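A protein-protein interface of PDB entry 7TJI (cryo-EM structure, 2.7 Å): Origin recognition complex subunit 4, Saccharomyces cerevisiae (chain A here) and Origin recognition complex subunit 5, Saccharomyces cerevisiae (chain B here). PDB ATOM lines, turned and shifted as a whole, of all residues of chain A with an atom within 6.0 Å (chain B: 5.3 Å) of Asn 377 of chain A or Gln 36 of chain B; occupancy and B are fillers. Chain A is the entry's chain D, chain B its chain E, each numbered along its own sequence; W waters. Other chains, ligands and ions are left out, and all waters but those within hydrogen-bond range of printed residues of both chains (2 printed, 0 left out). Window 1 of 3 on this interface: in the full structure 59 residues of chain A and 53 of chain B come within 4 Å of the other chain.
Of the 9 printed residues of chain A, 5 touch a printed residue of chain B.
Of the 17 printed residues of chain B, 7 touch a printed residue of chain A.
Hydrophobic or aromatic side chains of chain B within 4 Å of the printed part of chain A: Tyr 38, Met 188 and Pro 190.
Among the printed residues, no Asp or Glu carboxylate lies within 4 Å of a Lys or Arg side-chain nitrogen of the other chain.
O of Tyr 38 of chain B lies within hydrogen-bond range of NZ of Lys 43 of chain B (2.6 Å).
O of Asn 378 of chain A lies close to NE of Arg 382 of chain A (3.4 Å).
The backbone carbonyl oxygen (O) of Leu 171 of chain B lies within hydrogen-bond range of the side-chain amide nitrogen (NE2) of Gln 36 of chain B, at 3.1 Å.
OG1 of Thr 173 of chain B is in hydrogen-bond range of OH of Tyr 38 of chain B (2.9 Å).
O of Asn 377 of chain A sits at hydrogen-bond distance from NE of Arg 382 of chain A (2.9 Å).
O of Asn 373 of chain A sits at hydrogen-bond distance from OG of Ser 376 of chain A, at 2.8 Å.
Among the printed residues, pairs that only touch across the chains: Ser 376 of chain A with Met 188 of chain B (3.6 Å), Ser 376 of chain A with Pro 190 of chain B (3.98 Å), Asn 377 of chain A with Met 188 of chain B (3.6 Å), Asn 377 of chain A with Pro 190 of chain B (3.4 Å) and Arg 382 of chain A with Thr 173 of chain B (3.6 Å).
OE1 of Gln 374 of chain A sits close to O of Thr 186 of chain B (3.0 Å).
The side-chain amide nitrogen (ND2) of Asn 377 of chain A lies within hydrogen-bond range of the backbone carbonyl oxygen (O) of Phe 189 of chain B (3.5 Å).
O of Met 188 of chain B sits at hydrogen-bond distance from ND2 of Asn 373 of chain A, at 3.0 Å.
NE2 of Gln 374 of chain A lies close to SD of Met 188 of chain B (3.6 Å).
The backbone carbonyl oxygen (O) of Asn 377 of chain A sits at hydrogen-bond distance from the side-chain hydroxyl (OG1) of Thr 173 of chain B, 2.9 Å away.
NE of Arg 382 of chain A is in hydrogen-bond range of OH of Tyr 38 of chain B, at 3.3 Å.
The side-chain amide oxygen (OE1) of Gln 36 of chain B sits at hydrogen-bond distance from the side-chain amide nitrogen (ND2) of Asn 377 of chain A.
Water W1 lies within hydrogen-bond range of the backbone carbonyl oxygen of Phe 189 of chain B (2.7 Å), the backbone NH of Tyr 38 of chain B (2.8 Å) and the side-chain amide oxygen of Asn 377 of chain A (2.9 Å).
Water W2 lies within hydrogen-bond range of the backbone carbonyl oxygen of Ser 376 of chain A, the side-chain amide oxygen of Asn 377 of chain A and the backbone NH of Arg 191 of chain B.
Gln 36 of chain B touches just one residue of chain A: Asn 377.
Of the printed residues of chain A, Pro 190 of chain B touches Ser 376 (3.98 Å) and Asn 377 (3.4 Å).
Of the printed residues of chain A, Thr 173 of chain B touches Asn 377 (2.9 Å) and Arg 382 (3.6 Å).
Of the printed residues of chain B, Gln 374 of chain A touches Thr 186 and Met 188.
Leu 375 of chain A touches none of the printed residues of chain B.
The nearest residue of chain B that does not touch Asn 377 of chain A is Gly 37 of chain B (4.1 Å).
The nearest printed residue of chain A that does not touch Gln 36 of chain B is Asn 378 of chain A (6.4 Å).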
ATOM      1  N   ASN A 373      19.876  -3.662 -15.273  1.00  0.00           N
ATOM      2  CA  ASN A 373      21.032  -3.274 -14.470  1.00  0.00           C
ATOM      3  C   ASN A 373      21.897  -4.468 -14.090  1.00  0.00           C
ATOM      4  O   ASN A 373      23.122  -4.335 -14.021  1.00  0.00           O
ATOM      5  CB  ASN A 373      20.597  -2.531 -13.213  1.00  0.00           C
ATOM      6  CG  ASN A 373      21.780  -2.093 -12.363  1.00  0.00           C
ATOM      7  OD1 ASN A 373      22.070  -2.689 -11.329  1.00  0.00           O
ATOM      8  ND2 ASN A 373      22.466  -1.051 -12.802  1.00  0.00           N
ATOM      9  N   GLN A 374      21.292  -5.639 -13.862  1.00  0.00           N
ATOM     10  CA  GLN A 374      22.058  -6.830 -13.494  1.00  0.00           C
ATOM     11  C   GLN A 374      22.997  -7.310 -14.597  1.00  0.00           C
ATOM     12  O   GLN A 374      23.940  -8.051 -14.307  1.00  0.00           O
ATOM     13  CB  GLN A 374      21.122  -7.978 -13.105  1.00  0.00           C
ATOM     14  CG  GLN A 374      20.344  -7.786 -11.811  1.00  0.00           C
ATOM     15  CD  GLN A 374      21.214  -7.388 -10.642  1.00  0.00           C
ATOM     16  OE1 GLN A 374      21.020  -6.335 -10.041  1.00  0.00           O
ATOM     17  NE2 GLN A 374      22.169  -8.236 -10.302  1.00  0.00           N
ATOM     18  N   LEU A 375      22.777  -6.897 -15.844  1.00  0.00           N
ATOM     19  CA  LEU A 375      23.594  -7.316 -16.972  1.00  0.00           C
ATOM     20  C   LEU A 375      24.486  -6.212 -17.519  1.00  0.00           C
ATOM     21  O   LEU A 375      25.194  -6.445 -18.501  1.00  0.00           O
ATOM     22  CB  LEU A 375      22.693  -7.844 -18.095  1.00  0.00           C
ATOM     23  CG  LEU A 375      21.766  -8.995 -17.713  1.00  0.00           C
ATOM     24  CD1 LEU A 375      20.545  -9.019 -18.606  1.00  0.00           C
ATOM     25  CD2 LEU A 375      22.508 -10.310 -17.770  1.00  0.00           C
ATOM     26  N   SER A 376      24.482  -5.026 -16.911  1.00  0.00           N
ATOM     27  CA  SER A 376      25.103  -3.857 -17.527  1.00  0.00           C
ATOM     28  C   SER A 376      26.628  -3.899 -17.500  1.00  0.00           C
ATOM     29  O   SER A 376      27.263  -3.174 -18.267  1.00  0.00           O
ATOM     30  CB  SER A 376      24.596  -2.584 -16.850  1.00  0.00           C
ATOM     31  OG  SER A 376      24.765  -2.643 -15.448  1.00  0.00           O
ATOM     32  N   ASN A 377      27.230  -4.732 -16.653  1.00  0.00           N
ATOM     33  CA  ASN A 377      28.677  -4.891 -16.616  1.00  0.00           C
ATOM     34  C   ASN A 377      29.121  -6.238 -17.166  1.00  0.00           C
ATOM     35  O   ASN A 377      30.243  -6.672 -16.901  1.00  0.00           O
ATOM     36  CB  ASN A 377      29.206  -4.695 -15.195  1.00  0.00           C
ATOM     37  CG  ASN A 377      29.173  -3.253 -14.764  1.00  0.00           C
ATOM     38  OD1 ASN A 377      29.596  -2.372 -15.503  1.00  0.00           O
ATOM     39  ND2 ASN A 377      28.675  -3.002 -13.565  1.00  0.00           N
ATOM     40  N   ASN A 378      28.267  -6.898 -17.940  1.00  0.00           N
ATOM     41  CA  ASN A 378      28.621  -8.137 -18.618  1.00  0.00           C
ATOM     42  C   ASN A 378      29.523  -7.826 -19.815  1.00  0.00           C
ATOM     43  O   ASN A 378      29.943  -6.688 -20.039  1.00  0.00           O
ATOM     44  CB  ASN A 378      27.362  -8.885 -19.045  1.00  0.00           C
ATOM     45  CG  ASN A 378      26.923  -9.922 -18.032  1.00  0.00           C
ATOM     46  OD1 ASN A 378      27.511 -10.049 -16.958  1.00  0.00           O
ATOM     47  ND2 ASN A 378      25.883 -10.669 -18.370  1.00  0.00           N
ATOM     48  N   LEU A 379      29.830  -8.860 -20.601  1.00  0.00           N
ATOM     49  CA  LEU A 379      30.643  -8.678 -21.800  1.00  0.00           C
ATOM     50  C   LEU A 379      29.926  -7.818 -22.835  1.00  0.00           C
ATOM     51  O   LEU A 379      30.559  -7.014 -23.529  1.00  0.00           O
ATOM     52  CB  LEU A 379      31.004 -10.039 -22.390  1.00  0.00           C
ATOM     53  CG  LEU A 379      32.397 -10.261 -22.984  1.00  0.00           C
ATOM     54  CD1 LEU A 379      33.460  -9.425 -22.289  1.00  0.00           C
ATOM     55  CD2 LEU A 379      32.749 -11.736 -22.918  1.00  0.00           C
ATOM     56  N   GLY A 381      27.618  -5.397 -22.214  1.00  0.00           N
ATOM     57  CA  GLY A 381      27.570  -4.011 -21.786  1.00  0.00           C
ATOM     58  C   GLY A 381      28.921  -3.337 -21.714  1.00  0.00           C
ATOM     59  O   GLY A 381      29.018  -2.122 -21.910  1.00  0.00           O
ATOM     60  N   ARG A 382      29.975  -4.102 -21.427  1.00  0.00           N
ATOM     61  CA  ARG A 382      31.323  -3.544 -21.410  1.00  0.00           C
ATOM     62  C   ARG A 382      31.797  -3.165 -22.807  1.00  0.00           C
ATOM     63  O   ARG A 382      32.598  -2.236 -22.952  1.00  0.00           O
ATOM     64  CB  ARG A 382      32.297  -4.537 -20.779  1.00  0.00           C
ATOM     65  CG  ARG A 382      32.504  -4.349 -19.292  1.00  0.00           C
ATOM     66  CD  ARG A 382      33.498  -5.348 -18.747  1.00  0.00           C
ATOM     67  NE  ARG A 382      32.833  -6.556 -18.278  1.00  0.00           N
ATOM     68  CZ  ARG A 382      33.244  -7.789 -18.533  1.00  0.00           C
ATOM     69  NH1 ARG A 382      34.342  -8.021 -19.229  1.00  0.00           N
ATOM     70  NH2 ARG A 382      32.533  -8.814 -18.079  1.00  0.00           N
ATOM     71  N   ILE B  34      26.351  -5.889  -2.266  1.00  0.00           N
ATOM     72  CA  ILE B  34      27.502  -5.750  -3.152  1.00  0.00           C
ATOM     73  C   ILE B  34      27.244  -4.600  -4.113  1.00  0.00           C
ATOM     74  O   ILE B  34      26.176  -4.528  -4.724  1.00  0.00           O
ATOM     75  CB  ILE B  34      27.791  -7.058  -3.915  1.00  0.00           C
ATOM     76  CG1 ILE B  34      28.149  -8.175  -2.937  1.00  0.00           C
ATOM     77  CG2 ILE B  34      28.926  -6.877  -4.916  1.00  0.00           C
ATOM     78  CD1 ILE B  34      28.287  -9.529  -3.579  1.00  0.00           C
ATOM     79  N   LEU B  35      28.203  -3.683  -4.213  1.00  0.00           N
ATOM     80  CA  LEU B  35      28.225  -2.670  -5.262  1.00  0.00           C
ATOM     81  C   LEU B  35      29.338  -3.036  -6.230  1.00  0.00           C
ATOM     82  O   LEU B  35      30.505  -3.091  -5.841  1.00  0.00           O
ATOM     83  CB  LEU B  35      28.454  -1.269  -4.695  1.00  0.00           C
ATOM     84  CG  LEU B  35      27.580  -0.750  -3.557  1.00  0.00           C
ATOM     85  CD1 LEU B  35      27.787   0.748  -3.386  1.00  0.00           C
ATOM     86  CD2 LEU B  35      26.120  -1.064  -3.809  1.00  0.00           C
ATOM     87  N   GLN B  36      28.987  -3.297  -7.483  1.00  0.00           N
ATOM     88  CA  GLN B  36      29.962  -3.758  -8.460  1.00  0.00           C
ATOM     89  C   GLN B  36      30.065  -2.766  -9.605  1.00  0.00           C
ATOM     90  O   GLN B  36      29.054  -2.388 -10.196  1.00  0.00           O
ATOM     91  CB  GLN B  36      29.606  -5.148  -8.990  1.00  0.00           C
ATOM     92  CG  GLN B  36      30.732  -5.815  -9.759  1.00  0.00           C
ATOM     93  CD  GLN B  36      30.632  -5.579 -11.251  1.00  0.00           C
ATOM     94  OE1 GLN B  36      29.540  -5.578 -11.812  1.00  0.00           O
ATOM     95  NE2 GLN B  36      31.770  -5.359 -11.897  1.00  0.00           N
ATOM     96  N   GLY B  37      31.287  -2.369  -9.921  1.00  0.00           N
ATOM     97  CA  GLY B  37      31.539  -1.496 -11.047  1.00  0.00           C
ATOM     98  C   GLY B  37      33.026  -1.328 -11.230  1.00  0.00           C
ATOM     99  O   GLY B  37      33.813  -1.605 -10.323  1.00  0.00           O
ATOM    100  N   TYR B  38      33.402  -0.854 -12.410  1.00  0.00           N
ATOM    101  CA  TYR B  38      34.811  -0.661 -12.711  1.00  0.00           C
ATOM    102  C   TYR B  38      35.272   0.699 -12.193  1.00  0.00           C
ATOM    103  O   TYR B  38      34.532   1.413 -11.511  1.00  0.00           O
ATOM    104  CB  TYR B  38      35.056  -0.849 -14.205  1.00  0.00           C
ATOM    105  CG  TYR B  38      34.950  -2.303 -14.587  1.00  0.00           C
ATOM    106  CD1 TYR B  38      36.045  -3.147 -14.478  1.00  0.00           C
ATOM    107  CD2 TYR B  38      33.737  -2.849 -14.998  1.00  0.00           C
ATOM    108  CE1 TYR B  38      35.946  -4.485 -14.801  1.00  0.00           C
ATOM    109  CE2 TYR B  38      33.626  -4.188 -15.316  1.00  0.00           C
ATOM    110  CZ  TYR B  38      34.736  -5.000 -15.217  1.00  0.00           C
ATOM    111  OH  TYR B  38      34.639  -6.330 -15.536  1.00  0.00           O
ATOM    112  N   LYS B  43      31.127   4.616  -7.565  1.00  0.00           N
ATOM    113  CA  LYS B  43      30.674   3.784  -6.452  1.00  0.00           C
ATOM    114  C   LYS B  43      30.942   4.454  -5.109  1.00  0.00           C
ATOM    115  O   LYS B  43      30.036   4.577  -4.272  1.00  0.00           O
ATOM    116  CB  LYS B  43      31.360   2.420  -6.513  1.00  0.00           C
ATOM    117  CG  LYS B  43      31.182   1.689  -7.829  1.00  0.00           C
ATOM    118  CD  LYS B  43      31.901   0.353  -7.823  1.00  0.00           C
ATOM    119  CE  LYS B  43      33.417   0.525  -7.745  1.00  0.00           C
ATOM    120  NZ  LYS B  43      34.033   1.175  -8.928  1.00  0.00           N
ATOM    121  N   MET B 170      33.101  -3.977  -5.367  1.00  0.00           N
ATOM    122  CA  MET B 170      33.859  -4.878  -6.220  1.00  0.00           C
ATOM    123  C   MET B 170      34.142  -4.239  -7.571  1.00  0.00           C
ATOM    124  O   MET B 170      33.369  -3.419  -8.066  1.00  0.00           O
ATOM    125  CB  MET B 170      33.120  -6.194  -6.433  1.00  0.00           C
ATOM    126  CG  MET B 170      33.513  -7.261  -5.459  1.00  0.00           C
ATOM    127  SD  MET B 170      32.243  -8.509  -5.267  1.00  0.00           S
ATOM    128  CE  MET B 170      32.443  -8.834  -3.529  1.00  0.00           C
ATOM    129  N   LEU B 171      35.262  -4.641  -8.166  1.00  0.00           N
ATOM    130  CA  LEU B 171      35.678  -4.168  -9.478  1.00  0.00           C
ATOM    131  C   LEU B 171      35.351  -5.153 -10.593  1.00  0.00           C
ATOM    132  O   LEU B 171      34.787  -4.766 -11.617  1.00  0.00           O
ATOM    133  CB  LEU B 171      37.182  -3.867  -9.478  1.00  0.00           C
ATOM    134  CG  LEU B 171      37.633  -2.546  -8.856  1.00  0.00           C
ATOM    135  CD1 LEU B 171      39.147  -2.506  -8.723  1.00  0.00           C
ATOM    136  CD2 LEU B 171      37.129  -1.362  -9.655  1.00  0.00           C
ATOM    137  N   GLU B 172      35.681  -6.426 -10.406  1.00  0.00           N
ATOM    138  CA  GLU B 172      35.669  -7.389 -11.496  1.00  0.00           C
ATOM    139  C   GLU B 172      34.337  -8.120 -11.585  1.00  0.00           C
ATOM    140  O   GLU B 172      33.773  -8.543 -10.574  1.00  0.00           O
ATOM    141  CB  GLU B 172      36.808  -8.396 -11.322  1.00  0.00           C
ATOM    142  CG  GLU B 172      38.276  -7.865 -11.329  1.00  0.00           C
ATOM    143  CD  GLU B 172      38.576  -6.553 -12.087  1.00  0.00           C
ATOM    144  OE1 GLU B 172      38.067  -6.295 -13.202  1.00  0.00           O
ATOM    145  OE2 GLU B 172      39.346  -5.745 -11.527  1.00  0.00           O
ATOM    146  N   THR B 173      33.848  -8.263 -12.815  1.00  0.00           N
ATOM    147  CA  THR B 173      32.616  -9.002 -13.062  1.00  0.00           C
ATOM    148  C   THR B 173      32.804 -10.498 -12.818  1.00  0.00           C
ATOM    149  O   THR B 173      31.904 -11.162 -12.291  1.00  0.00           O
ATOM    150  CB  THR B 173      32.140  -8.726 -14.491  1.00  0.00           C
ATOM    151  OG1 THR B 173      32.056  -7.311 -14.693  1.00  0.00           O
ATOM    152  CG2 THR B 173      30.783  -9.338 -14.758  1.00  0.00           C
ATOM    153  N   LEU B 176      32.739 -11.414  -9.137  1.00  0.00           N
ATOM    154  CA  LEU B 176      31.374 -11.401  -8.622  1.00  0.00           C
ATOM    155  C   LEU B 176      30.584 -12.611  -9.109  1.00  0.00           C
ATOM    156  O   LEU B 176      29.797 -13.196  -8.355  1.00  0.00           O
ATOM    157  CB  LEU B 176      30.680 -10.102  -9.026  1.00  0.00           C
ATOM    158  CG  LEU B 176      29.184  -9.973  -8.728  1.00  0.00           C
ATOM    159  CD1 LEU B 176      28.937  -9.866  -7.239  1.00  0.00           C
ATOM    160  CD2 LEU B 176      28.592  -8.794  -9.454  1.00  0.00           C
ATOM    161  N   THR B 186      22.959  -7.119  -5.347  1.00  0.00           N
ATOM    162  CA  THR B 186      24.067  -6.431  -5.991  1.00  0.00           C
ATOM    163  C   THR B 186      23.520  -5.284  -6.824  1.00  0.00           C
ATOM    164  O   THR B 186      22.558  -5.459  -7.576  1.00  0.00           O
ATOM    165  CB  THR B 186      24.883  -7.394  -6.869  1.00  0.00           C
ATOM    166  OG1 THR B 186      25.259  -8.543  -6.104  1.00  0.00           O
ATOM    167  CG2 THR B 186      26.141  -6.722  -7.386  1.00  0.00           C
ATOM    168  N   VAL B 187      24.126  -4.113  -6.674  1.00  0.00           N
ATOM    169  CA  VAL B 187      23.841  -2.946  -7.496  1.00  0.00           C
ATOM    170  C   VAL B 187      25.023  -2.732  -8.428  1.00  0.00           C
ATOM    171  O   VAL B 187      26.175  -2.668  -7.980  1.00  0.00           O
ATOM    172  CB  VAL B 187      23.584  -1.696  -6.637  1.00  0.00           C
ATOM    173  CG1 VAL B 187      23.082  -0.556  -7.504  1.00  0.00           C
ATOM    174  CG2 VAL B 187      22.595  -2.005  -5.531  1.00  0.00           C
ATOM    175  N   MET B 188      24.740  -2.627  -9.716  1.00  0.00           N
ATOM    176  CA  MET B 188      25.768  -2.451 -10.726  1.00  0.00           C
ATOM    177  C   MET B 188      25.917  -0.982 -11.088  1.00  0.00           C
ATOM    178  O   MET B 188      24.931  -0.254 -11.219  1.00  0.00           O
ATOM    179  CB  MET B 188      25.451  -3.266 -11.978  1.00  0.00           C
ATOM    180  CG  MET B 188      25.909  -4.704 -11.914  1.00  0.00           C
ATOM    181  SD  MET B 188      24.669  -5.759 -11.149  1.00  0.00           S
ATOM    182  CE  MET B 188      25.547  -7.308 -11.037  1.00  0.00           C
ATOM    183  N   PHE B 189      27.163  -0.564 -11.250  1.00  0.00           N
ATOM    184  CA  PHE B 189      27.525   0.793 -11.645  1.00  0.00           C
ATOM    185  C   PHE B 189      28.195   0.668 -13.004  1.00  0.00           C
ATOM    186  O   PHE B 189      29.397   0.363 -13.077  1.00  0.00           O
ATOM    187  CB  PHE B 189      28.473   1.434 -10.632  1.00  0.00           C
ATOM    188  CG  PHE B 189      27.821   1.842  -9.337  1.00  0.00           C
ATOM    189  CD1 PHE B 189      27.411   0.895  -8.407  1.00  0.00           C
ATOM    190  CD2 PHE B 189      27.650   3.180  -9.034  1.00  0.00           C
ATOM    191  CE1 PHE B 189      26.823   1.272  -7.225  1.00  0.00           C
ATOM    192  CE2 PHE B 189      27.064   3.565  -7.849  1.00  0.00           C
ATOM    193  CZ  PHE B 189      26.651   2.609  -6.944  1.00  0.00           C
ATOM    194  N   PRO B 190      27.471   0.854 -14.104  1.00  0.00           N
ATOM    195  CA  PRO B 190      28.095   0.718 -15.423  1.00  0.00           C
ATOM    196  C   PRO B 190      28.977   1.913 -15.751  1.00  0.00           C
ATOM    197  O   PRO B 190      28.934   2.956 -15.097  1.00  0.00           O
ATOM    198  CB  PRO B 190      26.902   0.623 -16.377  1.00  0.00           C
ATOM    199  CG  PRO B 190      25.785   1.262 -15.656  1.00  0.00           C
ATOM    200  CD  PRO B 190      26.020   1.079 -14.192  1.00  0.00           C
ATOM    201  N   ARG B 191      29.813   1.728 -16.768  1.00  0.00           N
ATOM    202  CA  ARG B 191      30.729   2.779 -17.187  1.00  0.00           C
ATOM    203  C   ARG B 191      29.962   3.934 -17.820  1.00  0.00           C
ATOM    204  O   ARG B 191      28.964   3.732 -18.515  1.00  0.00           O
ATOM    205  CB  ARG B 191      31.770   2.220 -18.157  1.00  0.00           C
ATOM    206  CG  ARG B 191      33.007   1.689 -17.454  1.00  0.00           C
ATOM    207  CD  ARG B 191      33.801   0.713 -18.302  1.00  0.00           C
ATOM    208  NE  ARG B 191      34.184   1.265 -19.597  1.00  0.00           N
ATOM    209  CZ  ARG B 191      35.239   2.038 -19.806  1.00  0.00           C
ATOM    210  NH1 ARG B 191      36.051   2.384 -18.821  1.00  0.00           N
ATOM    211  NH2 ARG B 191      35.484   2.480 -21.034  1.00  0.00           N
HETATM  212  O   HOH W   1      31.512  -0.546 -14.435  1.00  0.00           O
HETATM  213  O   HOH W   2      29.611  -1.321 -18.316  1.00  0.00           O
